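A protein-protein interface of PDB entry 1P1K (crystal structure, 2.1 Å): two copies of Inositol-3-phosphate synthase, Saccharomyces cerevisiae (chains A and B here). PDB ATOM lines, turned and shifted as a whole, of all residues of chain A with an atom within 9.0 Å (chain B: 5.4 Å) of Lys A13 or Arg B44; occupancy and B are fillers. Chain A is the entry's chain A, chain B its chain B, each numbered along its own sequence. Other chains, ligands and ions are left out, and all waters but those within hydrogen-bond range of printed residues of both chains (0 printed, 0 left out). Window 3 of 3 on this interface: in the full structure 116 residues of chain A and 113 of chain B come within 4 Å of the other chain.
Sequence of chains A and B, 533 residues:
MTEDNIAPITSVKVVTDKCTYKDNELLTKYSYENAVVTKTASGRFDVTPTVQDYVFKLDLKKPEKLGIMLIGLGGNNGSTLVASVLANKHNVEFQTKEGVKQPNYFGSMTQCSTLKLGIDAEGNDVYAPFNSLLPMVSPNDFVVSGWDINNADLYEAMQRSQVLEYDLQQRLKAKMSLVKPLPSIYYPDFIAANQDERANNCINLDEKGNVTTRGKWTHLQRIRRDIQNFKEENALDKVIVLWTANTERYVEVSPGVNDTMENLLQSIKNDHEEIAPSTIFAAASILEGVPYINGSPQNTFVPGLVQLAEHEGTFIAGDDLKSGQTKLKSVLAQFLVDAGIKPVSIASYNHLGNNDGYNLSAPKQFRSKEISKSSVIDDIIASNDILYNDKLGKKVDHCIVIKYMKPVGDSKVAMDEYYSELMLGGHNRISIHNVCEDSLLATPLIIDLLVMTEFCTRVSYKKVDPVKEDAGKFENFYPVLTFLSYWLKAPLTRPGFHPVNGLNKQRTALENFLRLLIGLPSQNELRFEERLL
The backbone carbonyl oxygen (O) of Ser A11 is in hydrogen-bond range of the backbone NH (N) of Phe B45, 2.7 Å away. The backbone NH (N) of Lys A13 is in hydrogen-bond range of the backbone carbonyl oxygen (O) of Phe B45 (2.7 Å). The backbone carbonyl oxygen (O) of Lys A13 lies within hydrogen-bond range of the backbone NH (N) of Val B47 (2.9 Å). N of Val A15 sits at hydrogen-bond distance from O of Val B47.
O of Val A126 is in hydrogen-bond range of N of Leu A117. The backbone carbonyl oxygen (O) of Asp B46 lies within hydrogen-bond range of the backbone NH (N) of Thr B38 (2.9 Å). OG1 of Thr B40 sits close to N of Arg B44, 3.2 Å away. The guanidinium group (NE) of Arg B44 is in salt-bridge range of the side-chain carboxylate (OD1) of Asp B46 (2.8 Å).
Among the printed residues, merely in contact across the chains: Thr A10 with Gly B43, Ser A11 with Gly B43, Ser A11 with Arg B44, Val A12 with Phe B45, Lys A13 with Arg B44, Lys A13 with Asp B46, Val A14 with Val B47, Leu A117 with Phe B45, Val A126 with Phe B45 and Ala A128 with Phe B45.
No residue of chain A comes within 4 Å of Thr B40. Gly B43 touches just these residues of chain A: Thr A10 and Ser A11. Printed residues of chain B within 4 Å of Val A126: Phe B45. Of the printed residues of chain B, Thr A10 touches Gly B43. Gly A519 touches none of the printed residues of chain B. Thr A16 touches none of the printed residues of chain B. The nearest printed residue of chain B that does not touch Val A12 is Val B47 (4.02 Å).
Hydrophobic or aromatic side chains of chain B that line the printed part of chain A: Phe B45. Among the printed residues, no Asp or Glu carboxylate lies within 4 Å of a Lys or Arg side-chain nitrogen of the other chain.
No position is printed for both chains. Of the 14 pairs that touch across the chains among the printed residues, none has its exchanged pair printed and touching as well.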
ATOM      1  N   ILE A   9      14.426  16.426 -21.104  1.00  0.00           N
ATOM      2  CA  ILE A   9      13.147  17.116 -21.451  1.00  0.00           C
ATOM      3  C   ILE A   9      12.546  17.739 -20.195  1.00  0.00           C
ATOM      4  O   ILE A   9      12.605  17.145 -19.118  1.00  0.00           O
ATOM      5  CB  ILE A   9      12.110  16.121 -22.022  1.00  0.00           C
ATOM      6  CG1 ILE A   9      12.756  15.225 -23.085  1.00  0.00           C
ATOM      7  CG2 ILE A   9      10.939  16.887 -22.613  1.00  0.00           C
ATOM      8  CD1 ILE A   9      13.256  15.964 -24.307  1.00  0.00           C
ATOM      9  N   THR A  10      11.974  18.935 -20.325  1.00  0.00           N
ATOM     10  CA  THR A  10      11.355  19.588 -19.173  1.00  0.00           C
ATOM     11  C   THR A  10       9.930  19.061 -18.983  1.00  0.00           C
ATOM     12  O   THR A  10       9.223  18.773 -19.950  1.00  0.00           O
ATOM     13  CB  THR A  10      11.314  21.142 -19.319  1.00  0.00           C
ATOM     14  OG1 THR A  10      10.603  21.505 -20.506  1.00  0.00           O
ATOM     15  CG2 THR A  10      12.722  21.715 -19.385  1.00  0.00           C
ATOM     16  N   SER A  11       9.525  18.913 -17.727  1.00  0.00           N
ATOM     17  CA  SER A  11       8.191  18.422 -17.411  1.00  0.00           C
ATOM     18  C   SER A  11       7.661  19.151 -16.192  1.00  0.00           C
ATOM     19  O   SER A  11       8.383  19.905 -15.544  1.00  0.00           O
ATOM     20  CB  SER A  11       8.222  16.912 -17.145  1.00  0.00           C
ATOM     21  OG  SER A  11       9.113  16.589 -16.090  1.00  0.00           O
ATOM     22  N   VAL A  12       6.393  18.918 -15.885  1.00  0.00           N
ATOM     23  CA  VAL A  12       5.757  19.556 -14.748  1.00  0.00           C
ATOM     24  C   VAL A  12       4.965  18.542 -13.922  1.00  0.00           C
ATOM     25  O   VAL A  12       4.122  17.819 -14.457  1.00  0.00           O
ATOM     26  CB  VAL A  12       4.801  20.680 -15.223  1.00  0.00           C
ATOM     27  CG1 VAL A  12       4.175  21.380 -14.028  1.00  0.00           C
ATOM     28  CG2 VAL A  12       5.560  21.682 -16.073  1.00  0.00           C
ATOM     29  N   LYS A  13       5.249  18.479 -12.621  1.00  0.00           N
ATOM     30  CA  LYS A  13       4.524  17.576 -11.728  1.00  0.00           C
ATOM     31  C   LYS A  13       3.791  18.381 -10.662  1.00  0.00           C
ATOM     32  O   LYS A  13       4.410  18.889  -9.732  1.00  0.00           O
ATOM     33  CB  LYS A  13       5.464  16.594 -11.032  1.00  0.00           C
ATOM     34  CG  LYS A  13       4.739  15.751  -9.996  1.00  0.00           C
ATOM     35  CD  LYS A  13       5.623  14.677  -9.401  1.00  0.00           C
ATOM     36  CE  LYS A  13       4.818  13.767  -8.482  1.00  0.00           C
ATOM     37  NZ  LYS A  13       5.581  12.551  -8.071  1.00  0.00           N
ATOM     38  N   VAL A  14       2.476  18.496 -10.799  1.00  0.00           N
ATOM     39  CA  VAL A  14       1.679  19.243  -9.834  1.00  0.00           C
ATOM     40  C   VAL A  14       1.129  18.316  -8.754  1.00  0.00           C
ATOM     41  O   VAL A  14       0.324  17.433  -9.053  1.00  0.00           O
ATOM     42  CB  VAL A  14       0.469  19.921 -10.500  1.00  0.00           C
ATOM     43  CG1 VAL A  14      -0.381  20.571  -9.437  1.00  0.00           C
ATOM     44  CG2 VAL A  14       0.922  20.948 -11.523  1.00  0.00           C
ATOM     45  N   VAL A  15       1.550  18.511  -7.503  1.00  0.00           N
ATOM     46  CA  VAL A  15       1.045  17.673  -6.417  1.00  0.00           C
ATOM     47  C   VAL A  15      -0.325  18.219  -6.000  1.00  0.00           C
ATOM     48  O   VAL A  15      -0.434  19.195  -5.255  1.00  0.00           O
ATOM     49  CB  VAL A  15       2.033  17.632  -5.205  1.00  0.00           C
ATOM     50  CG1 VAL A  15       2.318  19.018  -4.698  1.00  0.00           C
ATOM     51  CG2 VAL A  15       1.460  16.789  -4.095  1.00  0.00           C
ATOM     52  N   THR A  16      -1.374  17.590  -6.523  1.00  0.00           N
ATOM     53  CA  THR A  16      -2.739  18.003  -6.245  1.00  0.00           C
ATOM     54  C   THR A  16      -3.591  16.759  -6.119  1.00  0.00           C
ATOM     55  O   THR A  16      -3.228  15.708  -6.637  1.00  0.00           O
ATOM     56  CB  THR A  16      -3.305  18.851  -7.385  1.00  0.00           C
ATOM     57  OG1 THR A  16      -4.680  19.156  -7.124  1.00  0.00           O
ATOM     58  CG2 THR A  16      -3.216  18.089  -8.691  1.00  0.00           C
ATOM     59  N   CYS A  19      -6.152  15.623  -9.493  1.00  0.00           N
ATOM     60  CA  CYS A  19      -5.698  14.827 -10.628  1.00  0.00           C
ATOM     61  C   CYS A  19      -5.292  13.403 -10.320  1.00  0.00           C
ATOM     62  O   CYS A  19      -4.497  13.153  -9.410  1.00  0.00           O
ATOM     63  CB  CYS A  19      -4.508  15.512 -11.292  1.00  0.00           C
ATOM     64  SG  CYS A  19      -4.881  17.136 -11.943  1.00  0.00           S
ATOM     65  N   TYR A  21      -4.254   9.509 -12.334  1.00  0.00           N
ATOM     66  CA  TYR A  21      -3.853   8.864 -13.567  1.00  0.00           C
ATOM     67  C   TYR A  21      -4.355   7.435 -13.671  1.00  0.00           C
ATOM     68  O   TYR A  21      -4.212   6.646 -12.741  1.00  0.00           O
ATOM     69  CB  TYR A  21      -2.332   8.902 -13.683  1.00  0.00           C
ATOM     70  CG  TYR A  21      -1.813  10.305 -13.853  1.00  0.00           C
ATOM     71  CD1 TYR A  21      -1.964  11.248 -12.839  1.00  0.00           C
ATOM     72  CD2 TYR A  21      -1.236  10.713 -15.054  1.00  0.00           C
ATOM     73  CE1 TYR A  21      -1.559  12.566 -13.020  1.00  0.00           C
ATOM     74  CE2 TYR A  21      -0.829  12.026 -15.246  1.00  0.00           C
ATOM     75  CZ  TYR A  21      -0.995  12.949 -14.226  1.00  0.00           C
ATOM     76  OH  TYR A  21      -0.617  14.259 -14.421  1.00  0.00           O
ATOM     77  N   LEU A 117       4.071  29.081 -13.933  1.00  0.00           N
ATOM     78  CA  LEU A 117       3.544  27.990 -13.117  1.00  0.00           C
ATOM     79  C   LEU A 117       3.313  28.431 -11.670  1.00  0.00           C
ATOM     80  O   LEU A 117       2.487  27.856 -10.956  1.00  0.00           O
ATOM     81  CB  LEU A 117       4.509  26.809 -13.109  1.00  0.00           C
ATOM     82  CG  LEU A 117       4.597  25.952 -14.369  1.00  0.00           C
ATOM     83  CD1 LEU A 117       5.520  24.766 -14.121  1.00  0.00           C
ATOM     84  CD2 LEU A 117       3.206  25.480 -14.727  1.00  0.00           C
ATOM     85  N   VAL A 126       7.982  31.822 -11.812  1.00  0.00           N
ATOM     86  CA  VAL A 126       8.598  30.679 -12.472  1.00  0.00           C
ATOM     87  C   VAL A 126       7.787  30.295 -13.703  1.00  0.00           C
ATOM     88  O   VAL A 126       6.583  30.036 -13.615  1.00  0.00           O
ATOM     89  CB  VAL A 126       8.686  29.476 -11.543  1.00  0.00           C
ATOM     90  CG1 VAL A 126       9.257  28.287 -12.295  1.00  0.00           C
ATOM     91  CG2 VAL A 126       9.556  29.828 -10.342  1.00  0.00           C
ATOM     92  N   ALA A 128       7.419  28.019 -17.510  1.00  0.00           N
ATOM     93  CA  ALA A 128       7.763  26.756 -18.139  1.00  0.00           C
ATOM     94  C   ALA A 128       7.240  26.809 -19.567  1.00  0.00           C
ATOM     95  O   ALA A 128       6.345  27.609 -19.884  1.00  0.00           O
ATOM     96  CB  ALA A 128       7.140  25.598 -17.385  1.00  0.00           C
ATOM     97  N   SER A 132       5.172  22.235 -22.108  1.00  0.00           N
ATOM     98  CA  SER A 132       5.829  21.361 -21.132  1.00  0.00           C
ATOM     99  C   SER A 132       4.859  20.879 -20.062  1.00  0.00           C
ATOM    100  O   SER A 132       5.155  19.943 -19.318  1.00  0.00           O
ATOM    101  CB  SER A 132       7.007  22.077 -20.457  1.00  0.00           C
ATOM    102  OG  SER A 132       6.562  23.177 -19.681  1.00  0.00           O
ATOM    103  N   LEU A 133       3.699  21.517 -19.985  1.00  0.00           N
ATOM    104  CA  LEU A 133       2.700  21.138 -18.993  1.00  0.00           C
ATOM    105  C   LEU A 133       2.075  19.778 -19.285  1.00  0.00           C
ATOM    106  O   LEU A 133       2.175  18.849 -18.481  1.00  0.00           O
ATOM    107  CB  LEU A 133       1.615  22.209 -18.913  1.00  0.00           C
ATOM    108  CG  LEU A 133       1.983  23.482 -18.144  1.00  0.00           C
ATOM    109  CD1 LEU A 133       3.220  24.146 -18.742  1.00  0.00           C
ATOM    110  CD2 LEU A 133       0.800  24.426 -18.182  1.00  0.00           C
ATOM    111  N   LEU A 134       1.440  19.665 -20.445  1.00  0.00           N
ATOM    112  CA  LEU A 134       0.790  18.427 -20.858  1.00  0.00           C
ATOM    113  C   LEU A 134       1.302  17.981 -22.228  1.00  0.00           C
ATOM    114  O   LEU A 134       1.698  18.803 -23.056  1.00  0.00           O
ATOM    115  CB  LEU A 134      -0.729  18.634 -20.885  1.00  0.00           C
ATOM    116  CG  LEU A 134      -1.320  18.999 -19.516  1.00  0.00           C
ATOM    117  CD1 LEU A 134      -2.719  19.541 -19.676  1.00  0.00           C
ATOM    118  CD2 LEU A 134      -1.299  17.778 -18.618  1.00  0.00           C
ATOM    119  N   ILE A 518      -3.945  20.429 -15.033  1.00  0.00           N
ATOM    120  CA  ILE A 518      -2.969  19.887 -14.091  1.00  0.00           C
ATOM    121  C   ILE A 518      -3.283  20.350 -12.659  1.00  0.00           C
ATOM    122  O   ILE A 518      -2.406  20.371 -11.797  1.00  0.00           O
ATOM    123  CB  ILE A 518      -1.500  20.275 -14.452  1.00  0.00           C
ATOM    124  CG1 ILE A 518      -1.323  21.795 -14.438  1.00  0.00           C
ATOM    125  CG2 ILE A 518      -1.133  19.698 -15.802  1.00  0.00           C
ATOM    126  CD1 ILE A 518       0.080  22.241 -14.820  1.00  0.00           C
ATOM    127  N   GLY A 519      -4.540  20.728 -12.422  1.00  0.00           N
ATOM    128  CA  GLY A 519      -4.973  21.158 -11.101  1.00  0.00           C
ATOM    129  C   GLY A 519      -4.516  22.512 -10.578  1.00  0.00           C
ATOM    130  O   GLY A 519      -4.446  22.711  -9.359  1.00  0.00           O
ATOM    131  N   LEU A 520      -4.207  23.446 -11.478  1.00  0.00           N
ATOM    132  CA  LEU A 520      -3.767  24.780 -11.082  1.00  0.00           C
ATOM    133  C   LEU A 520      -4.875  25.797 -11.304  1.00  0.00           C
ATOM    134  O   LEU A 520      -5.566  25.768 -12.324  1.00  0.00           O
ATOM    135  CB  LEU A 520      -2.517  25.194 -11.866  1.00  0.00           C
ATOM    136  CG  LEU A 520      -1.234  24.461 -11.464  1.00  0.00           C
ATOM    137  CD1 LEU A 520      -0.044  24.958 -12.281  1.00  0.00           C
ATOM    138  CD2 LEU A 520      -0.993  24.682  -9.975  1.00  0.00           C
ATOM    139  N   THR B  38       9.586  24.363  -7.825  1.00  0.00           N
ATOM    140  CA  THR B  38      10.991  24.017  -7.626  1.00  0.00           C
ATOM    141  C   THR B  38      11.478  23.122  -8.772  1.00  0.00           C
ATOM    142  O   THR B  38      11.087  21.959  -8.882  1.00  0.00           O
ATOM    143  CB  THR B  38      11.210  23.292  -6.272  1.00  0.00           C
ATOM    144  OG1 THR B  38      10.701  21.954  -6.342  1.00  0.00           O
ATOM    145  CG2 THR B  38      10.490  24.034  -5.154  1.00  0.00           C
ATOM    146  N   LYS B  39      12.328  23.672  -9.632  1.00  0.00           N
ATOM    147  CA  LYS B  39      12.850  22.914 -10.763  1.00  0.00           C
ATOM    148  C   LYS B  39      13.968  21.966 -10.344  1.00  0.00           C
ATOM    149  O   LYS B  39      15.098  22.391 -10.116  1.00  0.00           O
ATOM    150  CB  LYS B  39      13.349  23.875 -11.853  1.00  0.00           C
ATOM    151  CG  LYS B  39      13.988  23.191 -13.068  1.00  0.00           C
ATOM    152  CD  LYS B  39      13.827  24.012 -14.358  1.00  0.00           C
ATOM    153  CE  LYS B  39      14.419  25.417 -14.249  1.00  0.00           C
ATOM    154  NZ  LYS B  39      14.121  26.266 -15.445  1.00  0.00           N
ATOM    155  N   THR B  40      13.645  20.679 -10.240  1.00  0.00           N
ATOM    156  CA  THR B  40      14.631  19.675  -9.856  1.00  0.00           C
ATOM    157  C   THR B  40      15.815  19.748 -10.800  1.00  0.00           C
ATOM    158  O   THR B  40      15.742  20.384 -11.853  1.00  0.00           O
ATOM    159  CB  THR B  40      14.065  18.233  -9.924  1.00  0.00           C
ATOM    160  OG1 THR B  40      13.843  17.860 -11.289  1.00  0.00           O
ATOM    161  CG2 THR B  40      12.764  18.140  -9.163  1.00  0.00           C
ATOM    162  N   ALA B  41      16.903  19.085 -10.419  1.00  0.00           N
ATOM    163  CA  ALA B  41      18.118  19.071 -11.225  1.00  0.00           C
ATOM    164  C   ALA B  41      17.833  18.765 -12.701  1.00  0.00           C
ATOM    165  O   ALA B  41      18.216  19.537 -13.587  1.00  0.00           O
ATOM    166  CB  ALA B  41      19.099  18.053 -10.654  1.00  0.00           C
ATOM    167  N   SER B  42      17.152  17.649 -12.955  1.00  0.00           N
ATOM    168  CA  SER B  42      16.819  17.220 -14.319  1.00  0.00           C
ATOM    169  C   SER B  42      15.896  18.171 -15.084  1.00  0.00           C
ATOM    170  O   SER B  42      15.406  17.830 -16.166  1.00  0.00           O
ATOM    171  CB  SER B  42      16.190  15.818 -14.289  1.00  0.00           C
ATOM    172  OG  SER B  42      15.063  15.769 -13.424  1.00  0.00           O
ATOM    173  N   GLY B  43      15.662  19.354 -14.522  1.00  0.00           N
ATOM    174  CA  GLY B  43      14.805  20.330 -15.173  1.00  0.00           C
ATOM    175  C   GLY B  43      13.318  20.032 -15.076  1.00  0.00           C
ATOM    176  O   GLY B  43      12.539  20.465 -15.927  1.00  0.00           O
ATOM    177  N   ARG B  44      12.919  19.296 -14.041  1.00  0.00           N
ATOM    178  CA  ARG B  44      11.515  18.950 -13.837  1.00  0.00           C
ATOM    179  C   ARG B  44      10.902  19.954 -12.870  1.00  0.00           C
ATOM    180  O   ARG B  44      11.480  20.249 -11.828  1.00  0.00           O
ATOM    181  CB  ARG B  44      11.406  17.532 -13.275  1.00  0.00           C
ATOM    182  CG  ARG B  44       9.998  16.972 -13.221  1.00  0.00           C
ATOM    183  CD  ARG B  44       9.240  17.452 -12.000  1.00  0.00           C
ATOM    184  NE  ARG B  44       8.844  16.346 -11.128  1.00  0.00           N
ATOM    185  CZ  ARG B  44       9.691  15.599 -10.421  1.00  0.00           C
ATOM    186  NH1 ARG B  44      10.997  15.835 -10.476  1.00  0.00           N
ATOM    187  NH2 ARG B  44       9.229  14.614  -9.658  1.00  0.00           N
ATOM    188  N   PHE B  45       9.735  20.482 -13.222  1.00  0.00           N
ATOM    189  CA  PHE B  45       9.055  21.467 -12.388  1.00  0.00           C
ATOM    190  C   PHE B  45       8.081  20.841 -11.403  1.00  0.00           C
ATOM    191  O   PHE B  45       7.054  20.275 -11.797  1.00  0.00           O
ATOM    192  CB  PHE B  45       8.282  22.458 -13.256  1.00  0.00           C
ATOM    193  CG  PHE B  45       9.151  23.329 -14.107  1.00  0.00           C
ATOM    194  CD1 PHE B  45       9.885  24.362 -13.541  1.00  0.00           C
ATOM    195  CD2 PHE B  45       9.228  23.123 -15.480  1.00  0.00           C
ATOM    196  CE1 PHE B  45      10.683  25.182 -14.327  1.00  0.00           C
ATOM    197  CE2 PHE B  45      10.023  23.936 -16.279  1.00  0.00           C
ATOM    198  CZ  PHE B  45      10.753  24.969 -15.700  1.00  0.00           C
ATOM    199  N   ASP B  46       8.404  20.939 -10.118  1.00  0.00           N
ATOM    200  CA  ASP B  46       7.529  20.417  -9.087  1.00  0.00           C
ATOM    201  C   ASP B  46       6.726  21.576  -8.562  1.00  0.00           C
ATOM    202  O   ASP B  46       7.285  22.594  -8.148  1.00  0.00           O
ATOM    203  CB  ASP B  46       8.333  19.775  -7.977  1.00  0.00           C
ATOM    204  CG  ASP B  46       8.886  18.450  -8.389  1.00  0.00           C
ATOM    205  OD1 ASP B  46       8.078  17.565  -8.758  1.00  0.00           O
ATOM    206  OD2 ASP B  46      10.121  18.296  -8.357  1.00  0.00           O
ATOM    207  N   VAL B  47       5.407  21.420  -8.599  1.00  0.00           N
ATOM    208  CA  VAL B  47       4.510  22.470  -8.157  1.00  0.00           C
ATOM    209  C   VAL B  47       3.545  22.020  -7.068  1.00  0.00           C
ATOM    210  O   VAL B  47       2.816  21.032  -7.226  1.00  0.00           O
ATOM    211  CB  VAL B  47       3.697  23.009  -9.339  1.00  0.00           C
ATOM    212  CG1 VAL B  47       2.954  24.275  -8.936  1.00  0.00           C
ATOM    213  CG2 VAL B  47       4.625  23.277 -10.517  1.00  0.00           C
